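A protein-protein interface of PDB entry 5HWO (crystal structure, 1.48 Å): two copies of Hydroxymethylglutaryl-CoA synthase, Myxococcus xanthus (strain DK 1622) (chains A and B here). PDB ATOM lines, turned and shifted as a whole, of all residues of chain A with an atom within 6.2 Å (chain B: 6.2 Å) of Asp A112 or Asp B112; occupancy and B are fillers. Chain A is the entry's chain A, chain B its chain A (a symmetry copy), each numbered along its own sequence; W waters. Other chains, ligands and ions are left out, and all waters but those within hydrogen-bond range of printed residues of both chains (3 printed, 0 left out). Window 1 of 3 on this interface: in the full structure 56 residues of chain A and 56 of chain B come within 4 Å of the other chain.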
ATOM      1  N   LEU A  80      19.270   3.867   3.190  1.00  0.00           N
ATOM      2  CA  LEU A  80      19.212   3.195   1.900  1.00  0.00           C
ATOM      3  C   LEU A  80      18.160   2.114   2.022  1.00  0.00           C
ATOM      4  O   LEU A  80      18.342   1.144   2.778  1.00  0.00           O
ATOM      5  CB  LEU A  80      20.565   2.566   1.558  1.00  0.00           C
ATOM      6  CG  LEU A  80      20.645   1.732   0.287  1.00  0.00           C
ATOM      7  CD1 LEU A  80      20.366   2.583  -0.946  1.00  0.00           C
ATOM      8  CD2 LEU A  80      21.995   1.041   0.153  1.00  0.00           C
ATOM      9  N   VAL A  81      17.040   2.308   1.323  1.00  0.00           N
ATOM     10  CA  VAL A  81      15.901   1.407   1.404  1.00  0.00           C
ATOM     11  C   VAL A  81      15.590   0.915   0.002  1.00  0.00           C
ATOM     12  O   VAL A  81      15.583   1.704  -0.945  1.00  0.00           O
ATOM     13  CB  VAL A  81      14.671   2.119   2.002  1.00  0.00           C
ATOM     14  CG1 VAL A  81      13.466   1.198   2.006  1.00  0.00           C
ATOM     15  CG2 VAL A  81      14.951   2.571   3.436  1.00  0.00           C
ATOM     16  N   VAL A  82      15.348  -0.379  -0.137  1.00  0.00           N
ATOM     17  CA  VAL A  82      14.906  -0.951  -1.404  1.00  0.00           C
ATOM     18  C   VAL A  82      13.472  -1.444  -1.239  1.00  0.00           C
ATOM     19  O   VAL A  82      13.192  -2.302  -0.390  1.00  0.00           O
ATOM     20  CB  VAL A  82      15.829  -2.078  -1.880  1.00  0.00           C
ATOM     21  CG1 VAL A  82      15.275  -2.718  -3.121  1.00  0.00           C
ATOM     22  CG2 VAL A  82      17.254  -1.576  -2.150  1.00  0.00           C
ATOM     23  N   GLY A  83      12.564  -0.869  -2.022  1.00  0.00           N
ATOM     24  CA  GLY A  83      11.218  -1.401  -2.145  1.00  0.00           C
ATOM     25  C   GLY A  83      11.228  -2.431  -3.251  1.00  0.00           C
ATOM     26  O   GLY A  83      11.687  -2.155  -4.360  1.00  0.00           O
ATOM     27  N   THR A  84      10.761  -3.631  -2.937  1.00  0.00           N
ATOM     28  CA  THR A  84      10.758  -4.715  -3.904  1.00  0.00           C
ATOM     29  C   THR A  84       9.730  -5.749  -3.501  1.00  0.00           C
ATOM     30  O   THR A  84       9.416  -5.911  -2.319  1.00  0.00           O
ATOM     31  CB  THR A  84      12.155  -5.342  -4.044  1.00  0.00           C
ATOM     32  OG1 THR A  84      12.187  -6.289  -5.118  1.00  0.00           O
ATOM     33  CG2 THR A  84      12.604  -6.024  -2.777  1.00  0.00           C
ATOM     34  N   GLY A  87      12.355 -10.149  -3.845  1.00  0.00           N
ATOM     35  CA  GLY A  87      13.441 -10.369  -2.911  1.00  0.00           C
ATOM     36  C   GLY A  87      14.200 -11.638  -3.234  1.00  0.00           C
ATOM     37  O   GLY A  87      13.666 -12.578  -3.826  1.00  0.00           O
ATOM     38  N   ASP A  89      16.504 -13.037  -0.726  1.00  0.00           N
ATOM     39  CA  ASP A  89      16.869 -13.699   0.511  1.00  0.00           C
ATOM     40  C   ASP A  89      15.768 -13.400   1.515  1.00  0.00           C
ATOM     41  O   ASP A  89      15.196 -12.307   1.509  1.00  0.00           O
ATOM     42  CB  ASP A  89      18.224 -13.189   1.041  1.00  0.00           C
ATOM     43  CG  ASP A  89      18.860 -14.154   2.045  1.00  0.00           C
ATOM     44  OD1 ASP A  89      19.597 -15.063   1.597  1.00  0.00           O
ATOM     45  OD2 ASP A  89      18.635 -14.002   3.281  1.00  0.00           O
ATOM     46  N   LYS A  92      18.659 -11.367   4.337  1.00  0.00           N
ATOM     47  CA  LYS A  92      19.614 -10.374   3.901  1.00  0.00           C
ATOM     48  C   LYS A  92      18.933  -9.474   2.882  1.00  0.00           C
ATOM     49  O   LYS A  92      18.429  -9.977   1.866  1.00  0.00           O
ATOM     50  CB  LYS A  92      20.825 -11.039   3.254  1.00  0.00           C
ATOM     51  CG  LYS A  92      21.931 -10.056   2.855  1.00  0.00           C
ATOM     52  CD  LYS A  92      23.198 -10.795   2.419  1.00  0.00           C
ATOM     53  CE  LYS A  92      24.241  -9.861   1.814  1.00  0.00           C
ATOM     54  NZ  LYS A  92      24.602  -8.762   2.704  1.00  0.00           N
ATOM     55  N   PRO A  93      18.866  -8.170   3.114  1.00  0.00           N
ATOM     56  CA  PRO A  93      18.095  -7.312   2.212  1.00  0.00           C
ATOM     57  C   PRO A  93      18.870  -6.919   0.959  1.00  0.00           C
ATOM     58  O   PRO A  93      20.105  -6.839   0.943  1.00  0.00           O
ATOM     59  CB  PRO A  93      17.805  -6.079   3.080  1.00  0.00           C
ATOM     60  CG  PRO A  93      19.017  -6.008   4.001  1.00  0.00           C
ATOM     61  CD  PRO A  93      19.354  -7.440   4.300  1.00  0.00           C
ATOM     62  N   VAL A  94      18.112  -6.678  -0.115  1.00  0.00           N
ATOM     63  CA  VAL A  94      18.701  -6.097  -1.324  1.00  0.00           C
ATOM     64  C   VAL A  94      19.502  -4.842  -0.991  1.00  0.00           C
ATOM     65  O   VAL A  94      20.603  -4.627  -1.515  1.00  0.00           O
ATOM     66  CB  VAL A  94      17.607  -5.828  -2.371  1.00  0.00           C
ATOM     67  CG1 VAL A  94      18.189  -5.168  -3.609  1.00  0.00           C
ATOM     68  CG2 VAL A  94      16.914  -7.122  -2.755  1.00  0.00           C
ATOM     69  N   ALA A  95      18.997  -4.031  -0.063  1.00  0.00           N
ATOM     70  CA  ALA A  95      19.694  -2.813   0.323  1.00  0.00           C
ATOM     71  C   ALA A  95      21.111  -3.082   0.826  1.00  0.00           C
ATOM     72  O   ALA A  95      22.011  -2.278   0.580  1.00  0.00           O
ATOM     73  CB  ALA A  95      18.901  -2.106   1.412  1.00  0.00           C
ATOM     74  N   SER A  96      21.331  -4.187   1.550  1.00  0.00           N
ATOM     75  CA  SER A  96      22.693  -4.475   2.011  1.00  0.00           C
ATOM     76  C   SER A  96      23.618  -4.814   0.851  1.00  0.00           C
ATOM     77  O   SER A  96      24.767  -4.363   0.827  1.00  0.00           O
ATOM     78  CB  SER A  96      22.704  -5.567   3.101  1.00  0.00           C
ATOM     79  OG  SER A  96      22.413  -6.841   2.573  1.00  0.00           O
ATOM     80  N   THR A 110      19.919   0.443   6.583  1.00  0.00           N
ATOM     81  CA  THR A 110      19.636  -0.312   5.364  1.00  0.00           C
ATOM     82  C   THR A 110      18.521  -1.311   5.641  1.00  0.00           C
ATOM     83  O   THR A 110      18.536  -1.987   6.669  1.00  0.00           O
ATOM     84  CB  THR A 110      20.857  -1.078   4.837  1.00  0.00           C
ATOM     85  OG1 THR A 110      21.305  -2.003   5.831  1.00  0.00           O
ATOM     86  CG2 THR A 110      22.004  -0.150   4.485  1.00  0.00           C
ATOM     87  N   TYR A 111      17.552  -1.395   4.739  1.00  0.00           N
ATOM     88  CA  TYR A 111      16.500  -2.402   4.834  1.00  0.00           C
ATOM     89  C   TYR A 111      15.674  -2.369   3.559  1.00  0.00           C
ATOM     90  O   TYR A 111      15.776  -1.444   2.756  1.00  0.00           O
ATOM     91  CB  TYR A 111      15.614  -2.215   6.063  1.00  0.00           C
ATOM     92  CG  TYR A 111      14.843  -0.917   6.189  1.00  0.00           C
ATOM     93  CD1 TYR A 111      15.386   0.174   6.856  1.00  0.00           C
ATOM     94  CD2 TYR A 111      13.537  -0.805   5.714  1.00  0.00           C
ATOM     95  CE1 TYR A 111      14.680   1.343   7.008  1.00  0.00           C
ATOM     96  CE2 TYR A 111      12.819   0.361   5.873  1.00  0.00           C
ATOM     97  CZ  TYR A 111      13.388   1.429   6.547  1.00  0.00           C
ATOM     98  OH  TYR A 111      12.667   2.594   6.725  1.00  0.00           O
ATOM     99  N   ASP A 112      14.875  -3.417   3.374  1.00  0.00           N
ATOM    100  CA  ASP A 112      13.918  -3.506   2.281  1.00  0.00           C
ATOM    101  C   ASP A 112      12.493  -3.356   2.817  1.00  0.00           C
ATOM    102  O   ASP A 112      12.186  -3.743   3.952  1.00  0.00           O
ATOM    103  CB  ASP A 112      14.015  -4.851   1.544  1.00  0.00           C
ATOM    104  CG  ASP A 112      15.367  -5.104   0.872  1.00  0.00           C
ATOM    105  OD1 ASP A 112      16.223  -4.168   0.788  1.00  0.00           O
ATOM    106  OD2 ASP A 112      15.528  -6.272   0.399  1.00  0.00           O
ATOM    107  N   THR A 113      11.614  -2.827   1.977  1.00  0.00           N
ATOM    108  CA  THR A 113      10.180  -2.727   2.273  1.00  0.00           C
ATOM    109  C   THR A 113       9.380  -3.563   1.288  1.00  0.00           C
ATOM    110  O   THR A 113       9.694  -3.602   0.101  1.00  0.00           O
ATOM    111  CB  THR A 113       9.713  -1.265   2.217  1.00  0.00           C
ATOM    112  OG1 THR A 113      10.244  -0.671   1.044  1.00  0.00           O
ATOM    113  CG2 THR A 113      10.206  -0.490   3.398  1.00  0.00           C
ATOM    114  N   GLN A 114       8.297  -4.179   1.772  1.00  0.00           N
ATOM    115  CA  GLN A 114       7.510  -5.106   0.966  1.00  0.00           C
ATOM    116  C   GLN A 114       6.023  -4.843   1.145  1.00  0.00           C
ATOM    117  O   GLN A 114       5.475  -4.991   2.250  1.00  0.00           O
ATOM    118  CB  GLN A 114       7.815  -6.568   1.301  1.00  0.00           C
ATOM    119  CG  GLN A 114       7.050  -7.531   0.387  1.00  0.00           C
ATOM    120  CD  GLN A 114       7.028  -8.945   0.916  1.00  0.00           C
ATOM    121  OE1 GLN A 114       8.051  -9.476   1.337  1.00  0.00           O
ATOM    122  NE2 GLN A 114       5.863  -9.570   0.879  1.00  0.00           N
ATOM    123  N   HIS A 115       5.378  -4.497   0.044  1.00  0.00           N
ATOM    124  CA  HIS A 115       3.938  -4.653  -0.116  1.00  0.00           C
ATOM    125  C   HIS A 115       3.628  -4.540  -1.595  1.00  0.00           C
ATOM    126  O   HIS A 115       3.257  -3.466  -2.066  1.00  0.00           O
ATOM    127  CB  HIS A 115       3.093  -3.627   0.641  1.00  0.00           C
ATOM    128  CG  HIS A 115       1.629  -3.964   0.588  1.00  0.00           C
ATOM    129  ND1 HIS A 115       0.721  -3.527   1.523  1.00  0.00           N
ATOM    130  CD2 HIS A 115       0.938  -4.781  -0.244  1.00  0.00           C
ATOM    131  CE1 HIS A 115      -0.474  -4.030   1.255  1.00  0.00           C
ATOM    132  NE2 HIS A 115      -0.371  -4.799   0.190  1.00  0.00           N
ATOM    133  N   LEU B  80       0.460  -0.053  10.059  1.00  0.00           N
ATOM    134  CA  LEU B  80       0.650  -1.409  10.552  1.00  0.00           C
ATOM    135  C   LEU B  80       1.810  -1.994   9.776  1.00  0.00           C
ATOM    136  O   LEU B  80       1.705  -2.206   8.556  1.00  0.00           O
ATOM    137  CB  LEU B  80      -0.608  -2.250  10.317  1.00  0.00           C
ATOM    138  CG  LEU B  80      -0.537  -3.727  10.681  1.00  0.00           C
ATOM    139  CD1 LEU B  80      -0.301  -3.913  12.175  1.00  0.00           C
ATOM    140  CD2 LEU B  80      -1.794  -4.471  10.251  1.00  0.00           C
ATOM    141  N   VAL B  81       2.931  -2.201  10.470  1.00  0.00           N
ATOM    142  CA  VAL B  81       4.159  -2.673   9.850  1.00  0.00           C
ATOM    143  C   VAL B  81       4.585  -3.947  10.559  1.00  0.00           C
ATOM    144  O   VAL B  81       4.545  -4.014  11.788  1.00  0.00           O
ATOM    145  CB  VAL B  81       5.274  -1.613   9.948  1.00  0.00           C
ATOM    146  CG1 VAL B  81       6.574  -2.143   9.374  1.00  0.00           C
ATOM    147  CG2 VAL B  81       4.882  -0.344   9.190  1.00  0.00           C
ATOM    148  N   VAL B  82       4.976  -4.953   9.794  1.00  0.00           N
ATOM    149  CA  VAL B  82       5.535  -6.178  10.355  1.00  0.00           C
ATOM    150  C   VAL B  82       7.007  -6.264   9.963  1.00  0.00           C
ATOM    151  O   VAL B  82       7.343  -6.280   8.771  1.00  0.00           O
ATOM    152  CB  VAL B  82       4.766  -7.424   9.899  1.00  0.00           C
ATOM    153  CG1 VAL B  82       5.443  -8.668  10.401  1.00  0.00           C
ATOM    154  CG2 VAL B  82       3.308  -7.402  10.375  1.00  0.00           C
ATOM    155  N   GLY B  83       7.878  -6.275  10.967  1.00  0.00           N
ATOM    156  CA  GLY B  83       9.280  -6.594  10.756  1.00  0.00           C
ATOM    157  C   GLY B  83       9.434  -8.093  10.868  1.00  0.00           C
ATOM    158  O   GLY B  83       8.996  -8.696  11.850  1.00  0.00           O
ATOM    159  N   THR B  84      10.019  -8.699   9.845  1.00  0.00           N
ATOM    160  CA  THR B  84      10.185 -10.142   9.820  1.00  0.00           C
ATOM    161  C   THR B  84      11.304 -10.505   8.869  1.00  0.00           C
ATOM    162  O   THR B  84      11.582  -9.786   7.905  1.00  0.00           O
ATOM    163  CB  THR B  84       8.876 -10.849   9.436  1.00  0.00           C
ATOM    164  OG1 THR B  84       8.997 -12.269   9.580  1.00  0.00           O
ATOM    165  CG2 THR B  84       8.450 -10.536   8.024  1.00  0.00           C
ATOM    166  N   GLY B  87       9.207 -14.229   6.022  1.00  0.00           N
ATOM    167  CA  GLY B  87       8.113 -13.877   5.139  1.00  0.00           C
ATOM    168  C   GLY B  87       7.516 -15.104   4.483  1.00  0.00           C
ATOM    169  O   GLY B  87       8.177 -16.127   4.303  1.00  0.00           O
ATOM    170  N   ASP B  89       5.276 -14.677   1.593  1.00  0.00           N
ATOM    171  CA  ASP B  89       4.933 -14.360   0.220  1.00  0.00           C
ATOM    172  C   ASP B  89       5.948 -13.339  -0.265  1.00  0.00           C
ATOM    173  O   ASP B  89       6.393 -12.485   0.505  1.00  0.00           O
ATOM    174  CB  ASP B  89       3.507 -13.783   0.117  1.00  0.00           C
ATOM    175  CG  ASP B  89       2.939 -13.874  -1.302  1.00  0.00           C
ATOM    176  OD1 ASP B  89       2.330 -14.921  -1.622  1.00  0.00           O
ATOM    177  OD2 ASP B  89       3.091 -12.900  -2.095  1.00  0.00           O
ATOM    178  N   LYS B  92       2.725 -10.273  -1.085  1.00  0.00           N
ATOM    179  CA  LYS B  92       1.686  -9.955  -0.134  1.00  0.00           C
ATOM    180  C   LYS B  92       2.305  -9.915   1.254  1.00  0.00           C
ATOM    181  O   LYS B  92       2.907 -10.913   1.681  1.00  0.00           O
ATOM    182  CB  LYS B  92       0.586 -11.013  -0.163  1.00  0.00           C
ATOM    183  CG  LYS B  92      -0.604 -10.693   0.747  1.00  0.00           C
ATOM    184  CD  LYS B  92      -1.760 -11.667   0.510  1.00  0.00           C
ATOM    185  CE  LYS B  92      -2.874 -11.516   1.542  1.00  0.00           C
ATOM    186  NZ  LYS B  92      -3.394 -10.155   1.617  1.00  0.00           N
ATOM    187  N   PRO B  93       2.216  -8.803   1.971  1.00  0.00           N
ATOM    188  CA  PRO B  93       2.924  -8.705   3.249  1.00  0.00           C
ATOM    189  C   PRO B  93       2.166  -9.356   4.400  1.00  0.00           C
ATOM    190  O   PRO B  93       0.931  -9.447   4.412  1.00  0.00           O
ATOM    191  CB  PRO B  93       3.035  -7.188   3.461  1.00  0.00           C
ATOM    192  CG  PRO B  93       1.783  -6.648   2.779  1.00  0.00           C
ATOM    193  CD  PRO B  93       1.596  -7.523   1.574  1.00  0.00           C
ATOM    194  N   VAL B  94       2.938  -9.824   5.385  1.00  0.00           N
ATOM    195  CA  VAL B  94       2.342 -10.288   6.640  1.00  0.00           C
ATOM    196  C   VAL B  94       1.391  -9.240   7.211  1.00  0.00           C
ATOM    197  O   VAL B  94       0.297  -9.563   7.693  1.00  0.00           O
ATOM    198  CB  VAL B  94       3.444 -10.679   7.639  1.00  0.00           C
ATOM    199  CG1 VAL B  94       2.847 -11.105   8.969  1.00  0.00           C
ATOM    200  CG2 VAL B  94       4.294 -11.802   7.073  1.00  0.00           C
ATOM    201  N   ALA B  95       1.760  -7.965   7.103  1.00  0.00           N
ATOM    202  CA  ALA B  95       0.915  -6.897   7.614  1.00  0.00           C
ATOM    203  C   ALA B  95      -0.483  -6.911   7.001  1.00  0.00           C
ATOM    204  O   ALA B  95      -1.456  -6.594   7.686  1.00  0.00           O
ATOM    205  CB  ALA B  95       1.575  -5.556   7.330  1.00  0.00           C
ATOM    206  N   SER B  96      -0.610  -7.247   5.710  1.00  0.00           N
ATOM    207  CA  SER B  96      -1.950  -7.296   5.117  1.00  0.00           C
ATOM    208  C   SER B  96      -2.779  -8.432   5.697  1.00  0.00           C
ATOM    209  O   SER B  96      -3.969  -8.250   5.970  1.00  0.00           O
ATOM    210  CB  SER B  96      -1.886  -7.352   3.577  1.00  0.00           C
ATOM    211  OG  SER B  96      -1.432  -8.603   3.113  1.00  0.00           O
ATOM    212  N   THR B 110       0.050  -0.312   5.220  1.00  0.00           N
ATOM    213  CA  THR B 110       0.470  -1.656   5.614  1.00  0.00           C
ATOM    214  C   THR B 110       1.677  -2.068   4.783  1.00  0.00           C
ATOM    215  O   THR B 110       1.693  -1.864   3.570  1.00  0.00           O
ATOM    216  CB  THR B 110      -0.633  -2.707   5.428  1.00  0.00           C
ATOM    217  OG1 THR B 110      -1.018  -2.755   4.052  1.00  0.00           O
ATOM    218  CG2 THR B 110      -1.860  -2.400   6.265  1.00  0.00           C
ATOM    219  N   TYR B 111       2.688  -2.633   5.431  1.00  0.00           N
ATOM    220  CA  TYR B 111       3.841  -3.181   4.725  1.00  0.00           C
ATOM    221  C   TYR B 111       4.713  -3.929   5.718  1.00  0.00           C
ATOM    222  O   TYR B 111       4.544  -3.814   6.930  1.00  0.00           O
ATOM    223  CB  TYR B 111       4.646  -2.113   3.988  1.00  0.00           C
ATOM    224  CG  TYR B 111       5.260  -0.998   4.810  1.00  0.00           C
ATOM    225  CD1 TYR B 111       4.569   0.185   5.037  1.00  0.00           C
ATOM    226  CD2 TYR B 111       6.564  -1.093   5.292  1.00  0.00           C
ATOM    227  CE1 TYR B 111       5.131   1.217   5.748  1.00  0.00           C
ATOM    228  CE2 TYR B 111       7.139  -0.057   5.997  1.00  0.00           C
ATOM    229  CZ  TYR B 111       6.425   1.112   6.202  1.00  0.00           C
ATOM    230  OH  TYR B 111       7.002   2.160   6.893  1.00  0.00           O
ATOM    231  N   ASP B 112       5.633  -4.727   5.179  1.00  0.00           N
ATOM    232  CA  ASP B 112       6.641  -5.425   5.962  1.00  0.00           C
ATOM    233  C   ASP B 112       8.014  -4.793   5.734  1.00  0.00           C
ATOM    234  O   ASP B 112       8.313  -4.270   4.652  1.00  0.00           O
ATOM    235  CB  ASP B 112       6.728  -6.912   5.587  1.00  0.00           C
ATOM    236  CG  ASP B 112       5.443  -7.704   5.849  1.00  0.00           C
ATOM    237  OD1 ASP B 112       4.492  -7.177   6.507  1.00  0.00           O
ATOM    238  OD2 ASP B 112       5.436  -8.890   5.397  1.00  0.00           O
ATOM    239  N   THR B 113       8.865  -4.879   6.747  1.00  0.00           N
ATOM    240  CA  THR B 113      10.264  -4.445   6.661  1.00  0.00           C
ATOM    241  C   THR B 113      11.195  -5.631   6.853  1.00  0.00           C
ATOM    242  O   THR B 113      10.941  -6.498   7.683  1.00  0.00           O
ATOM    243  CB  THR B 113      10.567  -3.368   7.714  1.00  0.00           C
ATOM    244  OG1 THR B 113      10.024  -3.792   8.955  1.00  0.00           O
ATOM    245  CG2 THR B 113       9.938  -2.060   7.351  1.00  0.00           C
ATOM    246  N   GLN B 114      12.319  -5.628   6.127  1.00  0.00           N
ATOM    247  CA  GLN B 114      13.239  -6.760   6.125  1.00  0.00           C
ATOM    248  C   GLN B 114      14.678  -6.281   6.237  1.00  0.00           C
ATOM    249  O   GLN B 114      15.190  -5.578   5.351  1.00  0.00           O
ATOM    250  CB  GLN B 114      13.086  -7.629   4.874  1.00  0.00           C
ATOM    251  CG  GLN B 114      13.994  -8.862   4.925  1.00  0.00           C
ATOM    252  CD  GLN B 114      14.151  -9.528   3.580  1.00  0.00           C
ATOM    253  OE1 GLN B 114      13.176  -9.743   2.866  1.00  0.00           O
ATOM    254  NE2 GLN B 114      15.379  -9.877   3.234  1.00  0.00           N
ATOM    255  N   HIS B 115      15.328  -6.703   7.308  1.00  0.00           N
ATOM    256  CA  HIS B 115      16.781  -6.763   7.383  1.00  0.00           C
ATOM    257  C   HIS B 115      17.142  -7.649   8.559  1.00  0.00           C
ATOM    258  O   HIS B 115      17.411  -7.147   9.648  1.00  0.00           O
ATOM    259  CB  HIS B 115      17.473  -5.410   7.561  1.00  0.00           C
ATOM    260  CG  HIS B 115      18.965  -5.527   7.436  1.00  0.00           C
ATOM    261  ND1 HIS B 115      19.777  -4.474   7.086  1.00  0.00           N
ATOM    262  CD2 HIS B 115      19.780  -6.607   7.522  1.00  0.00           C
ATOM    263  CE1 HIS B 115      21.031  -4.886   6.994  1.00  0.00           C
ATOM    264  NE2 HIS B 115      21.063  -6.178   7.249  1.00  0.00           N
HETATM  265  O   HOH W   1      10.395  -6.243   3.424  1.00  0.00           O
HETATM  266  O   HOH W   2      14.083  -8.476   0.080  1.00  0.00           O
HETATM  267  O   HOH W   3       7.131 -10.546   4.200  1.00  0.00           O
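Of the 18 printed residues of chain B, 9 touch a printed residue of chain A.
Hydrophobic or aromatic side chains of chain B that line the printed part of chain A: Pro B93, Tyr B111 and His B115.
Along chain B the printed residues that touch a printed residue of chain A span positions 89 to 115.
Of the 18 printed residues of chain A, 9 touch a printed residue of chain B.
Among the printed residues, 19 pairs touch across the chains.
Among the printed residues, no Asp or Glu carboxylate lies within 4 Å of a Lys or Arg side-chain nitrogen of the other chain.
O of Asp A89 lies within hydrogen-bond range of NE2 of Gln B114 (3.0 Å).
The backbone carbonyl oxygen of Lys A92 sits at hydrogen-bond distance from the side-chain amide nitrogen of Gln B114 (3.3 Å).
The backbone carbonyl oxygen (O) of Thr A110 lies within hydrogen-bond range of a ring nitrogen (ND1) of His B115, at 2.8 Å.
The backbone carbonyl oxygen (O) of Asp A112 is in hydrogen-bond range of the backbone NH (N) of Gln B114 (2.9 Å).
NE2 of Gln A114 is in hydrogen-bond range of O of Asp B89, at 3.0 Å.
The side-chain amide nitrogen (NE2) of Gln A114 sits at hydrogen-bond distance from the backbone carbonyl oxygen (O) of Lys B92 (3.3 Å).
O of Asp B112 sits at hydrogen-bond distance from N of Gln A114 (2.9 Å).
ND1 of His A115 is in hydrogen-bond range of O of Thr B110, at 2.8 Å.
Of chain B, only Asp B112 (3.97 Å), Thr B113 (3.4 Å) and Gln B114 (2.9 Å) come within 4 Å of Asp A112.
Of the printed residues of chain A, Gln B114 touches Asp A89 (3.0 Å), Lys A92 (3.3 Å), Pro A93 (3.5 Å), Tyr A111 (3.5 Å) and Asp A112 (2.9 Å).
Of the printed residues of chain A, Thr B110 touches His A115.
Printed residues of chain B within 4 Å of Tyr A111: Gln B114 and His B115.
Gly B87 touches none of the printed residues of chain A.
The nearest residue of chain A that does not touch Asp B112 is His A115 (5.1 Å).
The nearest printed residue of chain B that does not touch Thr A110 is Gln B114 (5.1 Å).
Pro A93 touches His B115, and with the chains exchanged His A115 touches Pro B93.
Asp B112 touches its own counterpart, Asp A112.
Asp A112 touches Thr B113, and with the chains exchanged Thr A113 touches Asp B112.
Asp A112 touches Gln B114, and with the chains exchanged Gln A114 touches Asp B112.
Of the 19 pairs that touch across the chains among the printed residues, 19 have their exchanged pair printed and touching as well.
Among the printed residues, merely in contact across the chains: Pro A93 with Gln B114 (3.5 Å), Pro A93 with His B115 (3.4 Å), Tyr A111 with Gln B114 (3.5 Å), Tyr A111 with His B115 (3.99 Å), Asp A112 with Asp B112 (3.97 Å), Asp A112 with Thr B113 (3.4 Å), Thr A113 with Asp B112 (3.4 Å), Gln A114 with Pro B93 (3.5 Å), Gln A114 with Tyr B111 (3.5 Å), His A115 with Pro B93 (3.4 Å) and His A115 with Tyr B111 (3.99 Å).
Water W3 bridges OD2 of Asp B112 and OE1 of Gln A114.
Water W2 lies within hydrogen-bond range of the side-chain carboxylate of Asp A112 (2.7 Å) and the side-chain amide oxygen of Gln B114 (3.2 Å).
Water W1 lies within hydrogen-bond range of the backbone carbonyl oxygen (O) of Asp A112, the backbone carbonyl oxygen (O) of Asp B112, the backbone NH (N) of Gln A114 and the backbone NH (N) of Gln B114.
The backbone NH (N) of Val A94 sits at hydrogen-bond distance from the side-chain carboxylate (OD2) of Asp A112, 2.7 Å away.
The backbone NH of Tyr B111 is in hydrogen-bond range of the backbone carbonyl oxygen of Leu B80.
O of Tyr B111 sits at hydrogen-bond distance from N of Val B82 (3.1 Å).
The backbone carbonyl oxygen (O) of Thr B113 lies within hydrogen-bond range of the backbone NH (N) of Thr B84, 3.2 Å away.
NZ of Lys B92 is in hydrogen-bond range of OG of Ser B96.
The backbone NH (N) of Ala B95 sits at hydrogen-bond distance from the side-chain carboxylate (OD1) of Asp B112, 2.9 Å away.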
